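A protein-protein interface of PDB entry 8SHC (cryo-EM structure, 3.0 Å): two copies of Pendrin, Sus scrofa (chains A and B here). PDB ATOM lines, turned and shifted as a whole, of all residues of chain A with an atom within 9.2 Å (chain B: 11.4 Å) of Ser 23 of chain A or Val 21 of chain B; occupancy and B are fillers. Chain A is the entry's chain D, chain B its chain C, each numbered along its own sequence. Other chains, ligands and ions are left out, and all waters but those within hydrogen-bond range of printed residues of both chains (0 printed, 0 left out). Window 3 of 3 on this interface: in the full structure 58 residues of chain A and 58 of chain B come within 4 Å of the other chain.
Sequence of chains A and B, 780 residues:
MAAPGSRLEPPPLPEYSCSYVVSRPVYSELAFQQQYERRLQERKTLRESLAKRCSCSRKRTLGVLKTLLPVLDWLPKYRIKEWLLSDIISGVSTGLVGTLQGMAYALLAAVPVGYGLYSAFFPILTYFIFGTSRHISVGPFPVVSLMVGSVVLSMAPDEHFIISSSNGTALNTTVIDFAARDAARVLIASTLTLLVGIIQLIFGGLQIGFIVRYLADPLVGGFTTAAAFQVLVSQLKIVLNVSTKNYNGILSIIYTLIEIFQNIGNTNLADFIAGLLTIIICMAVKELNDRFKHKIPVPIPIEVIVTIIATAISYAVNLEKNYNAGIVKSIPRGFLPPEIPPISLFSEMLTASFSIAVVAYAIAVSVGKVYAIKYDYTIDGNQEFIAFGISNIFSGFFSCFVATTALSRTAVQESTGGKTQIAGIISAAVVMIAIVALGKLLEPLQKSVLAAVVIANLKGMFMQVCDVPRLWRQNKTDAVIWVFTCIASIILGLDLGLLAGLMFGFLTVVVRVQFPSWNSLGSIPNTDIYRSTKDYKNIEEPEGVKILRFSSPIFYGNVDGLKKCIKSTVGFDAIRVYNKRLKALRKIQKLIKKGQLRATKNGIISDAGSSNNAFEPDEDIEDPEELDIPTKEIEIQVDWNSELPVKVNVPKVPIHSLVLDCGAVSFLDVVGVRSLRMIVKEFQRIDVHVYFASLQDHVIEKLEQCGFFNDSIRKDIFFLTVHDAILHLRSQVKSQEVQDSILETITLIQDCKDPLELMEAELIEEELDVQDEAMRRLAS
The backbone carbonyl oxygen (O) of Arg 24 of chain B sits at hydrogen-bond distance from the backbone NH (N) of Tyr 20 of chain A, at 2.6 Å. The side-chain carboxylate (OD2) of Asp 528 of chain B is in hydrogen-bond range of the side-chain hydroxyl (OH) of Tyr 20 of chain A (2.7 Å). N of Tyr 20 of chain B is in hydrogen-bond range of O of Arg 24 of chain A (2.6 Å). The guanidinium group (NE) of Arg 24 of chain A is in salt-bridge range of the side-chain carboxylate (OD1) of Asp 528 of chain B. The side-chain carboxylate (OD2) of Asp 528 of chain A is in hydrogen-bond range of the side-chain hydroxyl (OH) of Tyr 20 of chain B, 2.7 Å away. The side-chain carboxylate (OD1) of Asp 528 of chain A is in salt-bridge range of the guanidinium group (NE) of Arg 24 of chain B (3.3 Å). The backbone carbonyl oxygen (O) of Val 22 of chain B sits close to the backbone carbonyl oxygen (O) of Tyr 20 of chain A. The backbone carbonyl oxygen (O) of Val 22 of chain A sits close to the backbone carbonyl oxygen (O) of Tyr 20 of chain B (3.5 Å).
The guanidinium group of Arg 24 of chain A lies within salt-bridge range of the side-chain carboxylate of Asp 724 of chain A, 2.7 Å away. The backbone carbonyl oxygen of Ile 524 of chain B sits at hydrogen-bond distance from the side-chain hydroxyl of Thr 527 of chain B. N of Ile 524 of chain B lies within hydrogen-bond range of O of Ile 529 of chain B (2.8 Å).
Among the printed residues, merely in contact across the chains: Tyr 20 of chain A with Ser 23 of chain B (3.4 Å), Tyr 20 of chain A with His 723 of chain B (3.1 Å), Val 21 of chain A with Val 22 of chain B (3.8 Å), Val 21 of chain A with Ser 23 of chain B (3.97 Å), Val 22 of chain A with Val 21 of chain B (3.8 Å), Val 22 of chain A with Val 22 of chain B (3.7 Å), Val 22 of chain A with Asp 528 of chain B (3.9 Å), Ser 23 of chain A with Tyr 20 of chain B (3.4 Å), Ser 23 of chain A with Val 21 of chain B (3.97 Å), Ser 23 of chain A with Asn 526 of chain B (3.99 Å), Arg 24 of chain A with Ser 19 of chain B (3.6 Å), Arg 24 of chain A with Thr 527 of chain B (3.9 Å), Arg 24 of chain A with Ile 529 of chain B (3.98 Å), Val 26 of chain A with Cys 18 of chain B (3.6 Å), Asn 526 of chain A with Ser 23 of chain B (3.98 Å), Thr 527 of chain A with Arg 24 of chain B (3.9 Å), Asp 528 of chain A with Val 22 of chain B (3.9 Å), His 723 of chain A with Tyr 20 of chain B (3.1 Å), Asp 724 of chain A with Tyr 20 of chain B (3.4 Å) and Leu 727 of chain A with Ser 19 of chain B (3.4 Å).
Of the printed residues of chain B, Ser 23 of chain A touches Tyr 20, Val 21 and Asn 526. Of chain A, only Val 22 and Ser 23 come within 4 Å of Val 21 of chain B. Val 22 of chain A touches just these residues of chain B: Tyr 20, Val 21, Val 22 and Asp 528. Val 22 of chain B touches four residues of chain A. Of the printed residues of chain A, Thr 527 of chain B touches Arg 24. Of the printed residues of chain A, Ile 529 of chain B touches Arg 24 (3.98 Å). Printed residues of chain A within 4 Å of Asn 526 of chain B: Ser 23. Printed residues of chain B within 4 Å of Asn 526 of chain A: Ser 23. Arg 730 of chain A touches none of the printed residues of chain B. Tyr 27 of chain A touches none of the printed residues of chain B. The nearest printed residue of chain B that does not touch Ser 23 of chain A is Thr 527 of chain B (5.4 Å). The nearest printed residue of chain B that does not touch Asp 528 of chain A is Asp 528 of chain B (5.1 Å).
Of the 15 printed residues of chain A, 12 touch a printed residue of chain B. Hydrophobic or aromatic side chains of chain A that line the printed part of chain B: Tyr 20, Val 21, Val 22, Val 26, His 723 and Leu 727. Of the 17 printed residues of chain B, 12 touch a printed residue of chain A. Hydrophobic or aromatic side chains of chain B that line the printed part of chain A: Tyr 20, Val 21, Val 22, Ile 529 and His 723. Among the printed residues, Asp or Glu carboxylates within 4 Å of a Lys or Arg side-chain nitrogen of the other chain: Arg 24 of chain A with Asp 528 of chain B (3.3 Å) and Asp 528 of chain A with Arg 24 of chain B (3.3 Å).
Tyr 20 of chain A touches Ser 23 of chain B, and with the chains exchanged Ser 23 of chain A touches Tyr 20 of chain B. Val 21 of chain A touches Val 22 of chain B, and with the chains exchanged Val 22 of chain A touches Val 21 of chain B. Val 22 of chain A touches its own counterpart, Val 22 of chain B. Arg 24 of chain A touches Asp 528 of chain B, and with the chains exchanged Asp 528 of chain A touches Arg 24 of chain B. Positions printed for both chains: 20, 21, 22, 23, 24, 526, 527, 528, 723 and 727.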
ATOM      1  N   TYR A  20      18.824  -1.485  10.630  1.00  0.00           N
ATOM      2  CA  TYR A  20      19.043  -2.892  10.962  1.00  0.00           C
ATOM      3  C   TYR A  20      18.556  -3.725   9.782  1.00  0.00           C
ATOM      4  O   TYR A  20      17.352  -3.921   9.601  1.00  0.00           O
ATOM      5  CB  TYR A  20      18.316  -3.251  12.255  1.00  0.00           C
ATOM      6  CG  TYR A  20      18.626  -4.624  12.811  1.00  0.00           C
ATOM      7  CD1 TYR A  20      18.087  -5.769  12.239  1.00  0.00           C
ATOM      8  CD2 TYR A  20      19.446  -4.772  13.921  1.00  0.00           C
ATOM      9  CE1 TYR A  20      18.366  -7.023  12.748  1.00  0.00           C
ATOM     10  CE2 TYR A  20      19.726  -6.019  14.440  1.00  0.00           C
ATOM     11  CZ  TYR A  20      19.185  -7.141  13.850  1.00  0.00           C
ATOM     12  OH  TYR A  20      19.466  -8.387  14.363  1.00  0.00           O
ATOM     13  N   VAL A  21      19.495  -4.216   8.978  1.00  0.00           N
ATOM     14  CA  VAL A  21      19.190  -5.012   7.795  1.00  0.00           C
ATOM     15  C   VAL A  21      19.998  -6.301   7.859  1.00  0.00           C
ATOM     16  O   VAL A  21      21.218  -6.264   8.053  1.00  0.00           O
ATOM     17  CB  VAL A  21      19.497  -4.244   6.494  1.00  0.00           C
ATOM     18  CG1 VAL A  21      19.327  -5.152   5.286  1.00  0.00           C
ATOM     19  CG2 VAL A  21      18.604  -3.020   6.375  1.00  0.00           C
ATOM     20  N   VAL A  22      19.321  -7.434   7.697  1.00  0.00           N
ATOM     21  CA  VAL A  22      19.973  -8.739   7.721  1.00  0.00           C
ATOM     22  C   VAL A  22      19.158  -9.702   6.867  1.00  0.00           C
ATOM     23  O   VAL A  22      17.926  -9.632   6.829  1.00  0.00           O
ATOM     24  CB  VAL A  22      20.144  -9.258   9.168  1.00  0.00           C
ATOM     25  CG1 VAL A  22      18.795  -9.560   9.804  1.00  0.00           C
ATOM     26  CG2 VAL A  22      21.044 -10.486   9.196  1.00  0.00           C
ATOM     27  N   SER A  23      19.858 -10.589   6.162  1.00  0.00           N
ATOM     28  CA  SER A  23      19.225 -11.621   5.349  1.00  0.00           C
ATOM     29  C   SER A  23      19.978 -12.924   5.561  1.00  0.00           C
ATOM     30  O   SER A  23      21.187 -12.989   5.320  1.00  0.00           O
ATOM     31  CB  SER A  23      19.217 -11.238   3.866  1.00  0.00           C
ATOM     32  OG  SER A  23      18.293 -10.196   3.612  1.00  0.00           O
ATOM     33  N   ARG A  24      19.268 -13.955   6.009  1.00  0.00           N
ATOM     34  CA  ARG A  24      19.869 -15.251   6.282  1.00  0.00           C
ATOM     35  C   ARG A  24      18.765 -16.297   6.292  1.00  0.00           C
ATOM     36  O   ARG A  24      17.588 -15.958   6.454  1.00  0.00           O
ATOM     37  CB  ARG A  24      20.623 -15.243   7.622  1.00  0.00           C
ATOM     38  CG  ARG A  24      19.745 -14.966   8.833  1.00  0.00           C
ATOM     39  CD  ARG A  24      20.213 -15.754  10.047  1.00  0.00           C
ATOM     40  NE  ARG A  24      19.651 -15.239  11.289  1.00  0.00           N
ATOM     41  CZ  ARG A  24      18.723 -15.859  12.007  1.00  0.00           C
ATOM     42  NH1 ARG A  24      18.217 -17.021  11.627  1.00  0.00           N
ATOM     43  NH2 ARG A  24      18.293 -15.300  13.133  1.00  0.00           N
ATOM     44  N   PRO A  25      19.106 -17.570   6.108  1.00  0.00           N
ATOM     45  CA  PRO A  25      18.098 -18.625   6.236  1.00  0.00           C
ATOM     46  C   PRO A  25      17.682 -18.818   7.686  1.00  0.00           C
ATOM     47  O   PRO A  25      18.373 -18.412   8.623  1.00  0.00           O
ATOM     48  CB  PRO A  25      18.806 -19.872   5.692  1.00  0.00           C
ATOM     49  CG  PRO A  25      19.973 -19.355   4.913  1.00  0.00           C
ATOM     50  CD  PRO A  25      20.383 -18.091   5.595  1.00  0.00           C
ATOM     51  N   VAL A  26      16.528 -19.453   7.860  1.00  0.00           N
ATOM     52  CA  VAL A  26      16.042 -19.795   9.192  1.00  0.00           C
ATOM     53  C   VAL A  26      16.853 -20.972   9.716  1.00  0.00           C
ATOM     54  O   VAL A  26      16.956 -22.014   9.056  1.00  0.00           O
ATOM     55  CB  VAL A  26      14.541 -20.119   9.157  1.00  0.00           C
ATOM     56  CG1 VAL A  26      14.116 -20.811  10.439  1.00  0.00           C
ATOM     57  CG2 VAL A  26      13.734 -18.846   8.942  1.00  0.00           C
ATOM     58  N   TYR A  27      17.430 -20.811  10.903  1.00  0.00           N
ATOM     59  CA  TYR A  27      18.374 -21.773  11.456  1.00  0.00           C
ATOM     60  C   TYR A  27      17.798 -22.407  12.713  1.00  0.00           C
ATOM     61  O   TYR A  27      17.625 -21.730  13.733  1.00  0.00           O
ATOM     62  CB  TYR A  27      19.711 -21.104  11.773  1.00  0.00           C
ATOM     63  CG  TYR A  27      20.606 -20.908  10.572  1.00  0.00           C
ATOM     64  CD1 TYR A  27      21.024 -21.991   9.810  1.00  0.00           C
ATOM     65  CD2 TYR A  27      21.039 -19.642  10.205  1.00  0.00           C
ATOM     66  CE1 TYR A  27      21.844 -21.817   8.714  1.00  0.00           C
ATOM     67  CE2 TYR A  27      21.860 -19.459   9.109  1.00  0.00           C
ATOM     68  CZ  TYR A  27      22.259 -20.549   8.368  1.00  0.00           C
ATOM     69  OH  TYR A  27      23.076 -20.371   7.277  1.00  0.00           O
ATOM     70  N   ASN A 526       6.011  -5.424  12.175  1.00  0.00           N
ATOM     71  CA  ASN A 526       7.035  -5.100  11.181  1.00  0.00           C
ATOM     72  C   ASN A 526       8.451  -5.143  11.747  1.00  0.00           C
ATOM     73  O   ASN A 526       9.373  -4.573  11.157  1.00  0.00           O
ATOM     74  CB  ASN A 526       6.771  -3.734  10.534  1.00  0.00           C
ATOM     75  CG  ASN A 526       5.903  -3.833   9.296  1.00  0.00           C
ATOM     76  OD1 ASN A 526       6.108  -4.702   8.447  1.00  0.00           O
ATOM     77  ND2 ASN A 526       4.927  -2.939   9.184  1.00  0.00           N
ATOM     78  N   THR A 527       8.653  -5.814  12.879  1.00  0.00           N
ATOM     79  CA  THR A 527       9.979  -5.966  13.468  1.00  0.00           C
ATOM     80  C   THR A 527      10.124  -7.402  13.958  1.00  0.00           C
ATOM     81  O   THR A 527       9.254  -8.248  13.734  1.00  0.00           O
ATOM     82  CB  THR A 527      10.205  -4.960  14.607  1.00  0.00           C
ATOM     83  OG1 THR A 527       9.127  -5.048  15.545  1.00  0.00           O
ATOM     84  CG2 THR A 527      10.300  -3.537  14.071  1.00  0.00           C
ATOM     85  N   ASP A 528      11.239  -7.678  14.633  1.00  0.00           N
ATOM     86  CA  ASP A 528      11.485  -8.969  15.263  1.00  0.00           C
ATOM     87  C   ASP A 528      11.637  -8.822  16.773  1.00  0.00           C
ATOM     88  O   ASP A 528      12.420  -9.538  17.400  1.00  0.00           O
ATOM     89  CB  ASP A 528      12.717  -9.644  14.663  1.00  0.00           C
ATOM     90  CG  ASP A 528      13.926  -8.731  14.634  1.00  0.00           C
ATOM     91  OD1 ASP A 528      13.778  -7.533  14.951  1.00  0.00           O
ATOM     92  OD2 ASP A 528      15.028  -9.214  14.298  1.00  0.00           O
ATOM     93  N   HIS A 723      12.250 -15.699  16.567  1.00  0.00           N
ATOM     94  CA  HIS A 723      11.654 -15.269  15.309  1.00  0.00           C
ATOM     95  C   HIS A 723      11.765 -16.332  14.231  1.00  0.00           C
ATOM     96  O   HIS A 723      10.957 -16.328  13.296  1.00  0.00           O
ATOM     97  CB  HIS A 723      12.298 -13.971  14.808  1.00  0.00           C
ATOM     98  CG  HIS A 723      11.521 -13.290  13.724  1.00  0.00           C
ATOM     99  ND1 HIS A 723      12.119 -12.756  12.604  1.00  0.00           N
ATOM    100  CD2 HIS A 723      10.193 -13.061  13.584  1.00  0.00           C
ATOM    101  CE1 HIS A 723      11.196 -12.224  11.823  1.00  0.00           C
ATOM    102  NE2 HIS A 723      10.018 -12.395  12.395  1.00  0.00           N
ATOM    103  N   ASP A 724      12.742 -17.237  14.331  1.00  0.00           N
ATOM    104  CA  ASP A 724      12.848 -18.361  13.411  1.00  0.00           C
ATOM    105  C   ASP A 724      11.734 -19.369  13.650  1.00  0.00           C
ATOM    106  O   ASP A 724      11.226 -19.976  12.701  1.00  0.00           O
ATOM    107  CB  ASP A 724      14.216 -19.026  13.559  1.00  0.00           C
ATOM    108  CG  ASP A 724      15.362 -18.052  13.364  1.00  0.00           C
ATOM    109  OD1 ASP A 724      15.730 -17.790  12.202  1.00  0.00           O
ATOM    110  OD2 ASP A 724      15.892 -17.548  14.377  1.00  0.00           O
ATOM    111  N   LEU A 727       8.586 -17.966  12.011  1.00  0.00           N
ATOM    112  CA  LEU A 727       8.654 -18.113  10.560  1.00  0.00           C
ATOM    113  C   LEU A 727       8.463 -19.567  10.141  1.00  0.00           C
ATOM    114  O   LEU A 727       7.780 -19.851   9.150  1.00  0.00           O
ATOM    115  CB  LEU A 727       9.987 -17.573  10.043  1.00  0.00           C
ATOM    116  CG  LEU A 727      10.140 -16.051  10.037  1.00  0.00           C
ATOM    117  CD1 LEU A 727      11.491 -15.647   9.470  1.00  0.00           C
ATOM    118  CD2 LEU A 727       9.011 -15.400   9.255  1.00  0.00           C
ATOM    119  N   ARG A 730       4.842 -20.308  10.374  1.00  0.00           N
ATOM    120  CA  ARG A 730       4.125 -19.688   9.267  1.00  0.00           C
ATOM    121  C   ARG A 730       4.374 -20.397   7.943  1.00  0.00           C
ATOM    122  O   ARG A 730       3.531 -20.317   7.044  1.00  0.00           O
ATOM    123  CB  ARG A 730       4.510 -18.213   9.145  1.00  0.00           C
ATOM    124  CG  ARG A 730       4.041 -17.350  10.305  1.00  0.00           C
ATOM    125  CD  ARG A 730       4.457 -15.900  10.122  1.00  0.00           C
ATOM    126  NE  ARG A 730       4.030 -15.067  11.240  1.00  0.00           N
ATOM    127  CZ  ARG A 730       4.311 -13.777  11.363  1.00  0.00           C
ATOM    128  NH1 ARG A 730       5.023 -13.135  10.452  1.00  0.00           N
ATOM    129  NH2 ARG A 730       3.867 -13.115  12.428  1.00  0.00           N
ATOM    130  N   SER B  17      14.228 -22.755   1.441  1.00  0.00           N
ATOM    131  CA  SER B  17      12.979 -22.668   2.188  1.00  0.00           C
ATOM    132  C   SER B  17      12.726 -21.243   2.669  1.00  0.00           C
ATOM    133  O   SER B  17      13.030 -20.278   1.968  1.00  0.00           O
ATOM    134  CB  SER B  17      12.998 -23.631   3.379  1.00  0.00           C
ATOM    135  OG  SER B  17      11.709 -23.757   3.955  1.00  0.00           O
ATOM    136  N   CYS B  18      12.163 -21.122   3.868  1.00  0.00           N
ATOM    137  CA  CYS B  18      11.884 -19.814   4.442  1.00  0.00           C
ATOM    138  C   CYS B  18      13.179 -19.091   4.794  1.00  0.00           C
ATOM    139  O   CYS B  18      14.192 -19.707   5.137  1.00  0.00           O
ATOM    140  CB  CYS B  18      11.004 -19.956   5.683  1.00  0.00           C
ATOM    141  SG  CYS B  18      11.676 -21.054   6.952  1.00  0.00           S
ATOM    142  N   SER B  19      13.138 -17.764   4.705  1.00  0.00           N
ATOM    143  CA  SER B  19      14.296 -16.921   4.955  1.00  0.00           C
ATOM    144  C   SER B  19      13.987 -15.913   6.053  1.00  0.00           C
ATOM    145  O   SER B  19      12.827 -15.586   6.323  1.00  0.00           O
ATOM    146  CB  SER B  19      14.736 -16.188   3.681  1.00  0.00           C
ATOM    147  OG  SER B  19      13.661 -15.453   3.121  1.00  0.00           O
ATOM    148  N   TYR B  20      15.050 -15.418   6.684  1.00  0.00           N
ATOM    149  CA  TYR B  20      14.955 -14.448   7.773  1.00  0.00           C
ATOM    150  C   TYR B  20      15.289 -13.075   7.199  1.00  0.00           C
ATOM    151  O   TYR B  20      16.458 -12.754   6.969  1.00  0.00           O
ATOM    152  CB  TYR B  20      15.892 -14.834   8.913  1.00  0.00           C
ATOM    153  CG  TYR B  20      15.740 -14.020  10.179  1.00  0.00           C
ATOM    154  CD1 TYR B  20      16.237 -12.725  10.265  1.00  0.00           C
ATOM    155  CD2 TYR B  20      15.115 -14.555  11.297  1.00  0.00           C
ATOM    156  CE1 TYR B  20      16.105 -11.984  11.423  1.00  0.00           C
ATOM    157  CE2 TYR B  20      14.982 -13.824  12.459  1.00  0.00           C
ATOM    158  CZ  TYR B  20      15.476 -12.539  12.517  1.00  0.00           C
ATOM    159  OH  TYR B  20      15.341 -11.806  13.673  1.00  0.00           O
ATOM    160  N   VAL B  21      14.258 -12.265   6.965  1.00  0.00           N
ATOM    161  CA  VAL B  21      14.412 -10.932   6.396  1.00  0.00           C
ATOM    162  C   VAL B  21      13.688  -9.938   7.292  1.00  0.00           C
ATOM    163  O   VAL B  21      12.514 -10.135   7.623  1.00  0.00           O
ATOM    164  CB  VAL B  21      13.866 -10.859   4.955  1.00  0.00           C
ATOM    165  CG1 VAL B  21      13.888  -9.425   4.448  1.00  0.00           C
ATOM    166  CG2 VAL B  21      14.670 -11.765   4.035  1.00  0.00           C
ATOM    167  N   VAL B  22      14.386  -8.875   7.684  1.00  0.00           N
ATOM    168  CA  VAL B  22      13.811  -7.838   8.533  1.00  0.00           C
ATOM    169  C   VAL B  22      14.527  -6.525   8.246  1.00  0.00           C
ATOM    170  O   VAL B  22      15.732  -6.503   7.980  1.00  0.00           O
ATOM    171  CB  VAL B  22      13.894  -8.222  10.029  1.00  0.00           C
ATOM    172  CG1 VAL B  22      15.340  -8.262  10.504  1.00  0.00           C
ATOM    173  CG2 VAL B  22      13.071  -7.263  10.877  1.00  0.00           C
ATOM    174  N   SER B  23      13.768  -5.430   8.275  1.00  0.00           N
ATOM    175  CA  SER B  23      14.315  -4.090   8.089  1.00  0.00           C
ATOM    176  C   SER B  23      13.668  -3.165   9.106  1.00  0.00           C
ATOM    177  O   SER B  23      12.441  -3.036   9.135  1.00  0.00           O
ATOM    178  CB  SER B  23      14.070  -3.581   6.665  1.00  0.00           C
ATOM    179  OG  SER B  23      14.892  -4.260   5.731  1.00  0.00           O
ATOM    180  N   ARG B  24      14.489  -2.526   9.932  1.00  0.00           N
ATOM    181  CA  ARG B  24      14.002  -1.632  10.972  1.00  0.00           C
ATOM    182  C   ARG B  24      15.143  -0.717  11.390  1.00  0.00           C
ATOM    183  O   ARG B  24      16.314  -1.030  11.147  1.00  0.00           O
ATOM    184  CB  ARG B  24      13.469  -2.421  12.180  1.00  0.00           C
ATOM    185  CG  ARG B  24      14.512  -3.284  12.874  1.00  0.00           C
ATOM    186  CD  ARG B  24      14.279  -3.330  14.376  1.00  0.00           C
ATOM    187  NE  ARG B  24      15.005  -4.422  15.013  1.00  0.00           N
ATOM    188  CZ  ARG B  24      16.062  -4.263  15.797  1.00  0.00           C
ATOM    189  NH1 ARG B  24      16.556  -3.064  16.056  1.00  0.00           N
ATOM    190  NH2 ARG B  24      16.638  -5.335  16.335  1.00  0.00           N
ATOM    191  N   SER B 523      30.824 -12.484  16.239  1.00  0.00           N
ATOM    192  CA  SER B 523      29.729 -12.614  15.287  1.00  0.00           C
ATOM    193  C   SER B 523      30.038 -13.636  14.200  1.00  0.00           C
ATOM    194  O   SER B 523      31.161 -13.714  13.698  1.00  0.00           O
ATOM    195  CB  SER B 523      29.424 -11.261  14.641  1.00  0.00           C
ATOM    196  OG  SER B 523      28.563 -11.414  13.524  1.00  0.00           O
ATOM    197  N   ILE B 524      29.025 -14.416  13.845  1.00  0.00           N
ATOM    198  CA  ILE B 524      29.092 -15.273  12.660  1.00  0.00           C
ATOM    199  C   ILE B 524      28.966 -14.394  11.420  1.00  0.00           C
ATOM    200  O   ILE B 524      28.051 -13.557  11.358  1.00  0.00           O
ATOM    201  CB  ILE B 524      27.992 -16.331  12.701  1.00  0.00           C
ATOM    202  CG1 ILE B 524      28.285 -17.370  13.787  1.00  0.00           C
ATOM    203  CG2 ILE B 524      27.838 -17.006  11.343  1.00  0.00           C
ATOM    204  CD1 ILE B 524      29.198 -18.491  13.340  1.00  0.00           C
ATOM    205  N   PRO B 525      29.855 -14.533  10.435  1.00  0.00           N
ATOM    206  CA  PRO B 525      29.854 -13.599   9.300  1.00  0.00           C
ATOM    207  C   PRO B 525      28.529 -13.596   8.548  1.00  0.00           C
ATOM    208  O   PRO B 525      27.885 -14.632   8.375  1.00  0.00           O
ATOM    209  CB  PRO B 525      30.998 -14.111   8.416  1.00  0.00           C
ATOM    210  CG  PRO B 525      31.259 -15.513   8.877  1.00  0.00           C
ATOM    211  CD  PRO B 525      30.935 -15.526  10.334  1.00  0.00           C
ATOM    212  N   ASN B 526      28.128 -12.399   8.112  1.00  0.00           N
ATOM    213  CA  ASN B 526      26.943 -12.166   7.285  1.00  0.00           C
ATOM    214  C   ASN B 526      25.641 -12.525   7.996  1.00  0.00           C
ATOM    215  O   ASN B 526      24.618 -12.752   7.341  1.00  0.00           O
ATOM    216  CB  ASN B 526      27.036 -12.918   5.953  1.00  0.00           C
ATOM    217  CG  ASN B 526      27.696 -12.095   4.864  1.00  0.00           C
ATOM    218  OD1 ASN B 526      27.396 -10.913   4.695  1.00  0.00           O
ATOM    219  ND2 ASN B 526      28.600 -12.718   4.117  1.00  0.00           N
ATOM    220  N   THR B 527      25.646 -12.572   9.326  1.00  0.00           N
ATOM    221  CA  THR B 527      24.442 -12.849  10.102  1.00  0.00           C
ATOM    222  C   THR B 527      24.434 -11.930  11.318  1.00  0.00           C
ATOM    223  O   THR B 527      25.278 -11.039  11.456  1.00  0.00           O
ATOM    224  CB  THR B 527      24.371 -14.327  10.518  1.00  0.00           C
ATOM    225  OG1 THR B 527      25.610 -14.715  11.119  1.00  0.00           O
ATOM    226  CG2 THR B 527      24.083 -15.222   9.319  1.00  0.00           C
ATOM    227  N   ASP B 528      23.466 -12.149  12.208  1.00  0.00           N
ATOM    228  CA  ASP B 528      23.383 -11.438  13.477  1.00  0.00           C
ATOM    229  C   ASP B 528      23.461 -12.406  14.651  1.00  0.00           C
ATOM    230  O   ASP B 528      22.822 -12.198  15.684  1.00  0.00           O
ATOM    231  CB  ASP B 528      22.105 -10.604  13.554  1.00  0.00           C
ATOM    232  CG  ASP B 528      20.865 -11.404  13.213  1.00  0.00           C
ATOM    233  OD1 ASP B 528      21.004 -12.567  12.783  1.00  0.00           O
ATOM    234  OD2 ASP B 528      19.748 -10.871  13.379  1.00  0.00           O
ATOM    235  N   ILE B 529      24.243 -13.473  14.502  1.00  0.00           N
ATOM    236  CA  ILE B 529      24.370 -14.521  15.507  1.00  0.00           C
ATOM    237  C   ILE B 529      25.747 -14.408  16.144  1.00  0.00           C
ATOM    238  O   ILE B 529      26.766 -14.420  15.442  1.00  0.00           O
ATOM    239  CB  ILE B 529      24.159 -15.916  14.893  1.00  0.00           C
ATOM    240  CG1 ILE B 529      22.778 -16.007  14.240  1.00  0.00           C
ATOM    241  CG2 ILE B 529      24.325 -16.995  15.952  1.00  0.00           C
ATOM    242  CD1 ILE B 529      22.699 -17.019  13.122  1.00  0.00           C
ATOM    243  N   HIS B 723      23.159  -6.619  18.403  1.00  0.00           N
ATOM    244  CA  HIS B 723      23.528  -6.248  17.043  1.00  0.00           C
ATOM    245  C   HIS B 723      23.300  -4.772  16.775  1.00  0.00           C
ATOM    246  O   HIS B 723      23.947  -4.215  15.882  1.00  0.00           O
ATOM    247  CB  HIS B 723      22.751  -7.076  16.014  1.00  0.00           C
ATOM    248  CG  HIS B 723      23.313  -7.000  14.628  1.00  0.00           C
ATOM    249  ND1 HIS B 723      22.521  -6.848  13.511  1.00  0.00           N
ATOM    250  CD2 HIS B 723      24.590  -7.048  14.178  1.00  0.00           C
ATOM    251  CE1 HIS B 723      23.283  -6.809  12.434  1.00  0.00           C
ATOM    252  NE2 HIS B 723      24.543  -6.929  12.810  1.00  0.00           N
ATOM    253  N   LEU B 727      26.163  -2.026  15.373  1.00  0.00           N
ATOM    254  CA  LEU B 727      25.875  -1.100  14.281  1.00  0.00           C
ATOM    255  C   LEU B 727      26.066   0.348  14.720  1.00  0.00           C
ATOM    256  O   LEU B 727      26.597   1.170  13.961  1.00  0.00           O
ATOM    257  CB  LEU B 727      24.452  -1.324  13.770  1.00  0.00           C
ATOM    258  CG  LEU B 727      24.226  -2.590  12.940  1.00  0.00           C
ATOM    259  CD1 LEU B 727      22.785  -2.675  12.467  1.00  0.00           C
ATOM    260  CD2 LEU B 727      25.185  -2.640  11.763  1.00  0.00           C
